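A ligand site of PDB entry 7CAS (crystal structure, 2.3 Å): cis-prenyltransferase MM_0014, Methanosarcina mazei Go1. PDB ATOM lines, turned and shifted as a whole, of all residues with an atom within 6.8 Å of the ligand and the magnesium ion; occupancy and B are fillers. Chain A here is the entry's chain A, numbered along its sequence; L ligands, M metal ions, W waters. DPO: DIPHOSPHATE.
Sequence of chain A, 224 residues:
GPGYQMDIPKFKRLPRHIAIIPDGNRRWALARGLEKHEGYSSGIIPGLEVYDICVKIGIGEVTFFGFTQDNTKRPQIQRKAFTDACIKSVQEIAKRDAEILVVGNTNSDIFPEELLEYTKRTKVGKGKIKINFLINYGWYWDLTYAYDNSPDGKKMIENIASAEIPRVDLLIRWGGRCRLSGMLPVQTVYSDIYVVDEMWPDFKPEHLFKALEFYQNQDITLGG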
ATOM      1  N   PRO A  22      23.915 -23.823 -11.885  1.00  0.00           N
ATOM      2  CA  PRO A  22      23.911 -25.270 -11.686  1.00  0.00           C
ATOM      3  C   PRO A  22      25.213 -25.916 -12.171  1.00  0.00           C
ATOM      4  O   PRO A  22      25.160 -26.721 -13.085  1.00  0.00           O
ATOM      5  CB  PRO A  22      22.707 -25.699 -12.531  1.00  0.00           C
ATOM      6  CG  PRO A  22      22.734 -24.740 -13.708  1.00  0.00           C
ATOM      7  CD  PRO A  22      23.260 -23.429 -13.139  1.00  0.00           C
ATOM      8  N   ASP A  23      26.346 -25.519 -11.588  1.00  0.00           N
ATOM      9  CA  ASP A  23      27.710 -25.917 -12.023  1.00  0.00           C
ATOM     10  C   ASP A  23      28.059 -27.270 -11.399  1.00  0.00           C
ATOM     11  O   ASP A  23      27.471 -27.596 -10.345  1.00  0.00           O
ATOM     12  CB  ASP A  23      28.728 -24.830 -11.643  1.00  0.00           C
ATOM     13  CG  ASP A  23      29.997 -24.825 -12.486  1.00  0.00           C
ATOM     14  OD1 ASP A  23      29.896 -25.068 -13.700  1.00  0.00           O
ATOM     15  OD2 ASP A  23      31.067 -24.517 -11.925  1.00  0.00           O
ATOM     16  N   GLY A  24      28.959 -28.022 -12.025  1.00  0.00           N
ATOM     17  CA  GLY A  24      29.590 -29.229 -11.441  1.00  0.00           C
ATOM     18  C   GLY A  24      29.245 -30.498 -12.219  1.00  0.00           C
ATOM     19  O   GLY A  24      29.631 -31.589 -11.757  1.00  0.00           O
ATOM     20  N   ASN A  25      28.595 -30.353 -13.379  1.00  0.00           N
ATOM     21  CA  ASN A  25      27.995 -31.480 -14.153  1.00  0.00           C
ATOM     22  C   ASN A  25      29.118 -32.400 -14.670  1.00  0.00           C
ATOM     23  O   ASN A  25      29.011 -33.610 -14.474  1.00  0.00           O
ATOM     24  CB  ASN A  25      27.117 -30.967 -15.291  1.00  0.00           C
ATOM     25  CG  ASN A  25      25.904 -30.205 -14.795  1.00  0.00           C
ATOM     26  OD1 ASN A  25      25.794 -29.000 -15.033  1.00  0.00           O
ATOM     27  ND2 ASN A  25      25.013 -30.884 -14.096  1.00  0.00           N
ATOM     28  N   ARG A  26      30.150 -31.823 -15.286  1.00  0.00           N
ATOM     29  CA  ARG A  26      31.285 -32.560 -15.911  1.00  0.00           C
ATOM     30  C   ARG A  26      32.070 -33.318 -14.819  1.00  0.00           C
ATOM     31  O   ARG A  26      32.348 -34.516 -15.033  1.00  0.00           O
ATOM     32  CB  ARG A  26      32.200 -31.611 -16.684  1.00  0.00           C
ATOM     33  CG  ARG A  26      31.591 -31.051 -17.956  1.00  0.00           C
ATOM     34  CD  ARG A  26      32.553 -30.171 -18.739  1.00  0.00           C
ATOM     35  NE  ARG A  26      32.985 -29.007 -17.978  1.00  0.00           N
ATOM     36  CZ  ARG A  26      33.841 -28.089 -18.413  1.00  0.00           C
ATOM     37  NH1 ARG A  26      34.351 -28.185 -19.628  1.00  0.00           N
ATOM     38  NH2 ARG A  26      34.168 -27.065 -17.638  1.00  0.00           N
ATOM     39  N   ARG A  27      32.397 -32.639 -13.714  1.00  0.00           N
ATOM     40  CA  ARG A  27      33.157 -33.220 -12.570  1.00  0.00           C
ATOM     41  C   ARG A  27      32.352 -34.361 -11.936  1.00  0.00           C
ATOM     42  O   ARG A  27      32.973 -35.336 -11.484  1.00  0.00           O
ATOM     43  CB  ARG A  27      33.487 -32.136 -11.538  1.00  0.00           C
ATOM     44  CG  ARG A  27      34.798 -31.398 -11.795  1.00  0.00           C
ATOM     45  CD  ARG A  27      34.974 -30.197 -10.884  1.00  0.00           C
ATOM     46  NE  ARG A  27      33.985 -29.161 -11.176  1.00  0.00           N
ATOM     47  CZ  ARG A  27      33.600 -28.216 -10.317  1.00  0.00           C
ATOM     48  NH1 ARG A  27      32.684 -27.324 -10.682  1.00  0.00           N
ATOM     49  NH2 ARG A  27      34.101 -28.179  -9.093  1.00  0.00           N
ATOM     50  N   TRP A  28      31.022 -34.213 -11.877  1.00  0.00           N
ATOM     51  CA  TRP A  28      30.086 -35.220 -11.312  1.00  0.00           C
ATOM     52  C   TRP A  28      30.112 -36.486 -12.180  1.00  0.00           C
ATOM     53  O   TRP A  28      30.121 -37.594 -11.596  1.00  0.00           O
ATOM     54  CB  TRP A  28      28.673 -34.638 -11.223  1.00  0.00           C
ATOM     55  CG  TRP A  28      27.644 -35.611 -10.751  1.00  0.00           C
ATOM     56  CD1 TRP A  28      27.248 -35.842  -9.461  1.00  0.00           C
ATOM     57  CD2 TRP A  28      26.837 -36.488 -11.566  1.00  0.00           C
ATOM     58  NE1 TRP A  28      26.263 -36.791  -9.421  1.00  0.00           N
ATOM     59  CE2 TRP A  28      25.995 -37.211 -10.695  1.00  0.00           C
ATOM     60  CE3 TRP A  28      26.753 -36.724 -12.944  1.00  0.00           C
ATOM     61  CZ2 TRP A  28      25.074 -38.152 -11.164  1.00  0.00           C
ATOM     62  CZ3 TRP A  28      25.851 -37.664 -13.400  1.00  0.00           C
ATOM     63  CH2 TRP A  28      25.029 -38.367 -12.519  1.00  0.00           C
ATOM     64  N   LYS A  36      32.737 -36.589 -19.622  1.00  0.00           N
ATOM     65  CA  LYS A  36      32.474 -35.190 -19.158  1.00  0.00           C
ATOM     66  C   LYS A  36      31.061 -34.766 -19.573  1.00  0.00           C
ATOM     67  O   LYS A  36      30.330 -34.235 -18.720  1.00  0.00           O
ATOM     68  CB  LYS A  36      33.529 -34.240 -19.735  1.00  0.00           C
ATOM     69  CG  LYS A  36      34.861 -34.223 -18.991  1.00  0.00           C
ATOM     70  CD  LYS A  36      35.818 -33.152 -19.474  1.00  0.00           C
ATOM     71  CE  LYS A  36      36.981 -32.914 -18.533  1.00  0.00           C
ATOM     72  NZ  LYS A  36      37.801 -31.752 -18.942  1.00  0.00           N
ATOM     73  N   TYR A  40      25.232 -33.573 -17.776  1.00  0.00           N
ATOM     74  CA  TYR A  40      24.271 -32.455 -17.948  1.00  0.00           C
ATOM     75  C   TYR A  40      22.829 -32.972 -17.839  1.00  0.00           C
ATOM     76  O   TYR A  40      21.998 -32.323 -17.181  1.00  0.00           O
ATOM     77  CB  TYR A  40      24.516 -31.754 -19.276  1.00  0.00           C
ATOM     78  CG  TYR A  40      25.839 -31.037 -19.371  1.00  0.00           C
ATOM     79  CD1 TYR A  40      26.094 -29.915 -18.607  1.00  0.00           C
ATOM     80  CD2 TYR A  40      26.824 -31.467 -20.238  1.00  0.00           C
ATOM     81  CE1 TYR A  40      27.300 -29.235 -18.692  1.00  0.00           C
ATOM     82  CE2 TYR A  40      28.041 -30.811 -20.337  1.00  0.00           C
ATOM     83  CZ  TYR A  40      28.284 -29.695 -19.563  1.00  0.00           C
ATOM     84  OH  TYR A  40      29.480 -29.035 -19.655  1.00  0.00           O
ATOM     85  N   ASN A  71      30.512 -20.601 -22.925  1.00  0.00           N
ATOM     86  CA  ASN A  71      30.297 -22.070 -22.754  1.00  0.00           C
ATOM     87  C   ASN A  71      30.269 -22.750 -24.123  1.00  0.00           C
ATOM     88  O   ASN A  71      30.372 -23.990 -24.169  1.00  0.00           O
ATOM     89  CB  ASN A  71      29.005 -22.372 -21.976  1.00  0.00           C
ATOM     90  CG  ASN A  71      29.154 -22.213 -20.479  1.00  0.00           C
ATOM     91  OD1 ASN A  71      30.258 -22.093 -19.967  1.00  0.00           O
ATOM     92  ND2 ASN A  71      28.037 -22.239 -19.764  1.00  0.00           N
ATOM     93  N   ARG A  74      33.564 -24.431 -25.590  1.00  0.00           N
ATOM     94  CA  ARG A  74      33.843 -25.812 -25.104  1.00  0.00           C
ATOM     95  C   ARG A  74      33.653 -26.802 -26.258  1.00  0.00           C
ATOM     96  O   ARG A  74      33.046 -26.460 -27.278  1.00  0.00           O
ATOM     97  CB  ARG A  74      32.937 -26.160 -23.918  1.00  0.00           C
ATOM     98  CG  ARG A  74      33.015 -25.168 -22.761  1.00  0.00           C
ATOM     99  CD  ARG A  74      33.154 -25.857 -21.419  1.00  0.00           C
ATOM    100  NE  ARG A  74      33.175 -24.907 -20.303  1.00  0.00           N
ATOM    101  CZ  ARG A  74      32.324 -24.904 -19.286  1.00  0.00           C
ATOM    102  NH1 ARG A  74      31.365 -25.818 -19.208  1.00  0.00           N
ATOM    103  NH2 ARG A  74      32.437 -24.004 -18.321  1.00  0.00           N
ATOM    104  N   GLN A  78      30.008 -31.606 -25.740  1.00  0.00           N
ATOM    105  CA  GLN A  78      29.569 -30.984 -24.460  1.00  0.00           C
ATOM    106  C   GLN A  78      28.453 -29.971 -24.736  1.00  0.00           C
ATOM    107  O   GLN A  78      27.426 -30.018 -24.023  1.00  0.00           O
ATOM    108  CB  GLN A  78      30.754 -30.324 -23.759  1.00  0.00           C
ATOM    109  CG  GLN A  78      31.679 -31.316 -23.061  1.00  0.00           C
ATOM    110  CD  GLN A  78      32.934 -30.657 -22.535  1.00  0.00           C
ATOM    111  OE1 GLN A  78      32.881 -29.630 -21.859  1.00  0.00           O
ATOM    112  NE2 GLN A  78      34.079 -31.243 -22.850  1.00  0.00           N
ATOM    113  N   PHE A  82      24.560 -29.962 -23.030  1.00  0.00           N
ATOM    114  CA  PHE A  82      24.078 -28.950 -22.044  1.00  0.00           C
ATOM    115  C   PHE A  82      23.006 -28.067 -22.699  1.00  0.00           C
ATOM    116  O   PHE A  82      22.121 -27.586 -21.983  1.00  0.00           O
ATOM    117  CB  PHE A  82      25.252 -28.146 -21.447  1.00  0.00           C
ATOM    118  CG  PHE A  82      25.990 -27.231 -22.395  1.00  0.00           C
ATOM    119  CD1 PHE A  82      25.331 -26.240 -23.104  1.00  0.00           C
ATOM    120  CD2 PHE A  82      27.382 -27.266 -22.467  1.00  0.00           C
ATOM    121  CE1 PHE A  82      26.024 -25.368 -23.925  1.00  0.00           C
ATOM    122  CE2 PHE A  82      28.074 -26.392 -23.279  1.00  0.00           C
ATOM    123  CZ  PHE A  82      27.396 -25.444 -24.013  1.00  0.00           C
ATOM    124  N   ARG A 173      25.129 -21.193  -6.036  1.00  0.00           N
ATOM    125  CA  ARG A 173      26.019 -21.832  -7.038  1.00  0.00           C
ATOM    126  C   ARG A 173      26.473 -23.202  -6.498  1.00  0.00           C
ATOM    127  O   ARG A 173      27.014 -23.250  -5.374  1.00  0.00           O
ATOM    128  CB  ARG A 173      27.226 -20.936  -7.333  1.00  0.00           C
ATOM    129  CG  ARG A 173      28.324 -21.622  -8.140  1.00  0.00           C
ATOM    130  CD  ARG A 173      29.102 -20.655  -9.000  1.00  0.00           C
ATOM    131  NE  ARG A 173      29.987 -21.341  -9.932  1.00  0.00           N
ATOM    132  CZ  ARG A 173      30.498 -20.790 -11.033  1.00  0.00           C
ATOM    133  NH1 ARG A 173      30.220 -19.538 -11.337  1.00  0.00           N
ATOM    134  NH2 ARG A 173      31.274 -21.509 -11.820  1.00  0.00           N
ATOM    135  N   TRP A 174      26.248 -24.252  -7.293  1.00  0.00           N
ATOM    136  CA  TRP A 174      26.736 -25.637  -7.024  1.00  0.00           C
ATOM    137  C   TRP A 174      28.117 -25.817  -7.646  1.00  0.00           C
ATOM    138  O   TRP A 174      28.469 -25.034  -8.541  1.00  0.00           O
ATOM    139  CB  TRP A 174      25.725 -26.671  -7.548  1.00  0.00           C
ATOM    140  CG  TRP A 174      24.560 -26.889  -6.635  1.00  0.00           C
ATOM    141  CD1 TRP A 174      24.349 -27.958  -5.813  1.00  0.00           C
ATOM    142  CD2 TRP A 174      23.445 -25.998  -6.421  1.00  0.00           C
ATOM    143  NE1 TRP A 174      23.186 -27.795  -5.103  1.00  0.00           N
ATOM    144  CE2 TRP A 174      22.607 -26.602  -5.460  1.00  0.00           C
ATOM    145  CE3 TRP A 174      23.080 -24.757  -6.941  1.00  0.00           C
ATOM    146  CZ2 TRP A 174      21.422 -26.009  -5.029  1.00  0.00           C
ATOM    147  CZ3 TRP A 174      21.905 -24.165  -6.508  1.00  0.00           C
ATOM    148  CH2 TRP A 174      21.097 -24.795  -5.558  1.00  0.00           C
ATOM    149  N   GLY A 175      28.893 -26.779  -7.142  1.00  0.00           N
ATOM    150  CA  GLY A 175      30.207 -27.164  -7.701  1.00  0.00           C
ATOM    151  C   GLY A 175      31.365 -26.449  -6.995  1.00  0.00           C
ATOM    152  O   GLY A 175      32.483 -26.519  -7.514  1.00  0.00           O
ATOM    153  N   ARG A 177      32.670 -23.559  -6.452  1.00  0.00           N
ATOM    154  CA  ARG A 177      33.374 -22.336  -6.932  1.00  0.00           C
ATOM    155  C   ARG A 177      32.562 -21.096  -6.539  1.00  0.00           C
ATOM    156  O   ARG A 177      31.345 -21.083  -6.797  1.00  0.00           O
ATOM    157  CB  ARG A 177      33.601 -22.396  -8.445  1.00  0.00           C
ATOM    158  CG  ARG A 177      34.071 -23.748  -8.970  1.00  0.00           C
ATOM    159  CD  ARG A 177      35.335 -23.657  -9.800  1.00  0.00           C
ATOM    160  NE  ARG A 177      35.133 -23.001 -11.083  1.00  0.00           N
ATOM    161  CZ  ARG A 177      35.839 -21.957 -11.536  1.00  0.00           C
ATOM    162  NH1 ARG A 177      35.579 -21.441 -12.726  1.00  0.00           N
ATOM    163  NH2 ARG A 177      36.813 -21.441 -10.795  1.00  0.00           N
ATOM    164  N   MET A 199      28.306 -31.041  -6.474  1.00  0.00           N
ATOM    165  CA  MET A 199      28.006 -30.760  -7.900  1.00  0.00           C
ATOM    166  C   MET A 199      26.484 -30.720  -8.085  1.00  0.00           C
ATOM    167  O   MET A 199      25.782 -31.302  -7.253  1.00  0.00           O
ATOM    168  CB  MET A 199      28.602 -31.841  -8.813  1.00  0.00           C
ATOM    169  CG  MET A 199      30.097 -32.048  -8.607  1.00  0.00           C
ATOM    170  SD  MET A 199      31.076 -30.539  -8.827  1.00  0.00           S
ATOM    171  CE  MET A 199      31.948 -30.488  -7.261  1.00  0.00           C
ATOM    172  N   TRP A 200      26.022 -30.064  -9.149  1.00  0.00           N
ATOM    173  CA  TRP A 200      24.595 -29.718  -9.394  1.00  0.00           C
ATOM    174  C   TRP A 200      23.749 -30.994  -9.430  1.00  0.00           C
ATOM    175  O   TRP A 200      22.669 -31.036  -8.830  1.00  0.00           O
ATOM    176  CB  TRP A 200      24.465 -28.895 -10.670  1.00  0.00           C
ATOM    177  CG  TRP A 200      23.055 -28.732 -11.164  1.00  0.00           C
ATOM    178  CD1 TRP A 200      22.533 -29.196 -12.333  1.00  0.00           C
ATOM    179  CD2 TRP A 200      21.992 -28.036 -10.498  1.00  0.00           C
ATOM    180  NE1 TRP A 200      21.218 -28.838 -12.450  1.00  0.00           N
ATOM    181  CE2 TRP A 200      20.854 -28.122 -11.333  1.00  0.00           C
ATOM    182  CE3 TRP A 200      21.877 -27.329  -9.290  1.00  0.00           C
ATOM    183  CZ2 TRP A 200      19.635 -27.536 -11.009  1.00  0.00           C
ATOM    184  CZ3 TRP A 200      20.666 -26.764  -8.960  1.00  0.00           C
ATOM    185  CH2 TRP A 200      19.559 -26.866  -9.807  1.00  0.00           C
HETATM  186  P1  DPO L   1      29.849 -27.576 -16.063  1.00  0.00           P
HETATM  187  O1  DPO L   1      28.553 -27.661 -15.280  1.00  0.00           O
HETATM  188  O2  DPO L   1      30.557 -26.239 -15.896  1.00  0.00           O
HETATM  189  O3  DPO L   1      29.691 -27.978 -17.500  1.00  0.00           O
HETATM  190  O4  DPO L   1      30.852 -28.674 -15.394  1.00  0.00           O
HETATM  191  P2  DPO L   1      32.064 -28.516 -14.357  1.00  0.00           P
HETATM  192  O5  DPO L   1      31.756 -27.254 -13.562  1.00  0.00           O
HETATM  193  O6  DPO L   1      32.058 -29.754 -13.500  1.00  0.00           O
HETATM  194  O7  DPO L   1      33.301 -28.383 -15.190  1.00  0.00           O
HETATM  195 MG    MG M   1      31.731 -25.592 -14.522  1.00  0.00          MG
HETATM  196  O   HOH W   1      31.806 -24.087 -15.548  1.00  0.00           O
HETATM  197  O   HOH W   2      33.118 -24.934 -13.450  1.00  0.00           O
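The magnesium ion is bound by water W1 (1.8 Å), water W2 (1.9 Å), an oxygen (O2) of the ligand (1.9 Å), an oxygen (O5) of the ligand (1.9 Å) and the side-chain carboxylate (OD1) of Asp 23 (2.1 Å).
The magnesium ion has five donor atoms within binding distance.
The side-chain carboxylate of Asp 23 is in salt-bridge range of the guanidinium group of Arg 27 (3.5 Å).
The guanidinium group (NH2) of Arg 173 lies within salt-bridge range of the side-chain carboxylate (OD2) of Asp 23 (3.0 Å).
The backbone carbonyl oxygen of Asp 23 sits at hydrogen-bond distance from the backbone NH of Trp 200, at 3.1 Å.
NH1 of Arg 26 sits at hydrogen-bond distance from OE1 of Gln 78, at 3.0 Å.
The guanidinium group (NH2) of Arg 27 lies within hydrogen-bond range of the backbone carbonyl oxygen (O) of Gly 175, 2.8 Å away.
The side-chain amide oxygen (OD1) of Asn 25 sits close to the backbone carbonyl oxygen (O) of Pro 22.
The guanidinium group of Arg 74 lies within hydrogen-bond range of the side-chain amide oxygen of Asn 71 (3.3 Å).
Of the 19 residues printed, 1 comes within 4 Å of the magnesium ion.
Hydrophobic or aromatic side chains that line the ligand: Tyr 40.
Of the 19 residues printed, 7 come within 4 Å of the ligand.
O3 of the ligand is in hydrogen-bond range of OH of Tyr 40, at 2.4 Å.
The backbone NH (N) of Arg 26 is in hydrogen-bond range of an oxygen (O4) of the ligand, at 3.2 Å.
NE of Arg 26 lies within salt-bridge range of O7 of the ligand (2.9 Å).
The backbone NH of Arg 27 lies within hydrogen-bond range of an oxygen (O6) of the ligand.
The guanidinium group (NE) of Arg 27 is in salt-bridge range of an oxygen (O6) of the ligand, 3.1 Å away.
The backbone NH (N) of Asn 25 sits at hydrogen-bond distance from an oxygen (O1) of the ligand, at 3.3 Å.
The side-chain amide oxygen of Asn 25 lies close to an oxygen (O1) of the ligand, at 3.1 Å.
The backbone NH (N) of Gly 24 lies within hydrogen-bond range of an oxygen (O1) of the ligand (3.3 Å).
NH1 of Arg 74 is in salt-bridge range of O3 of the ligand (3.2 Å).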
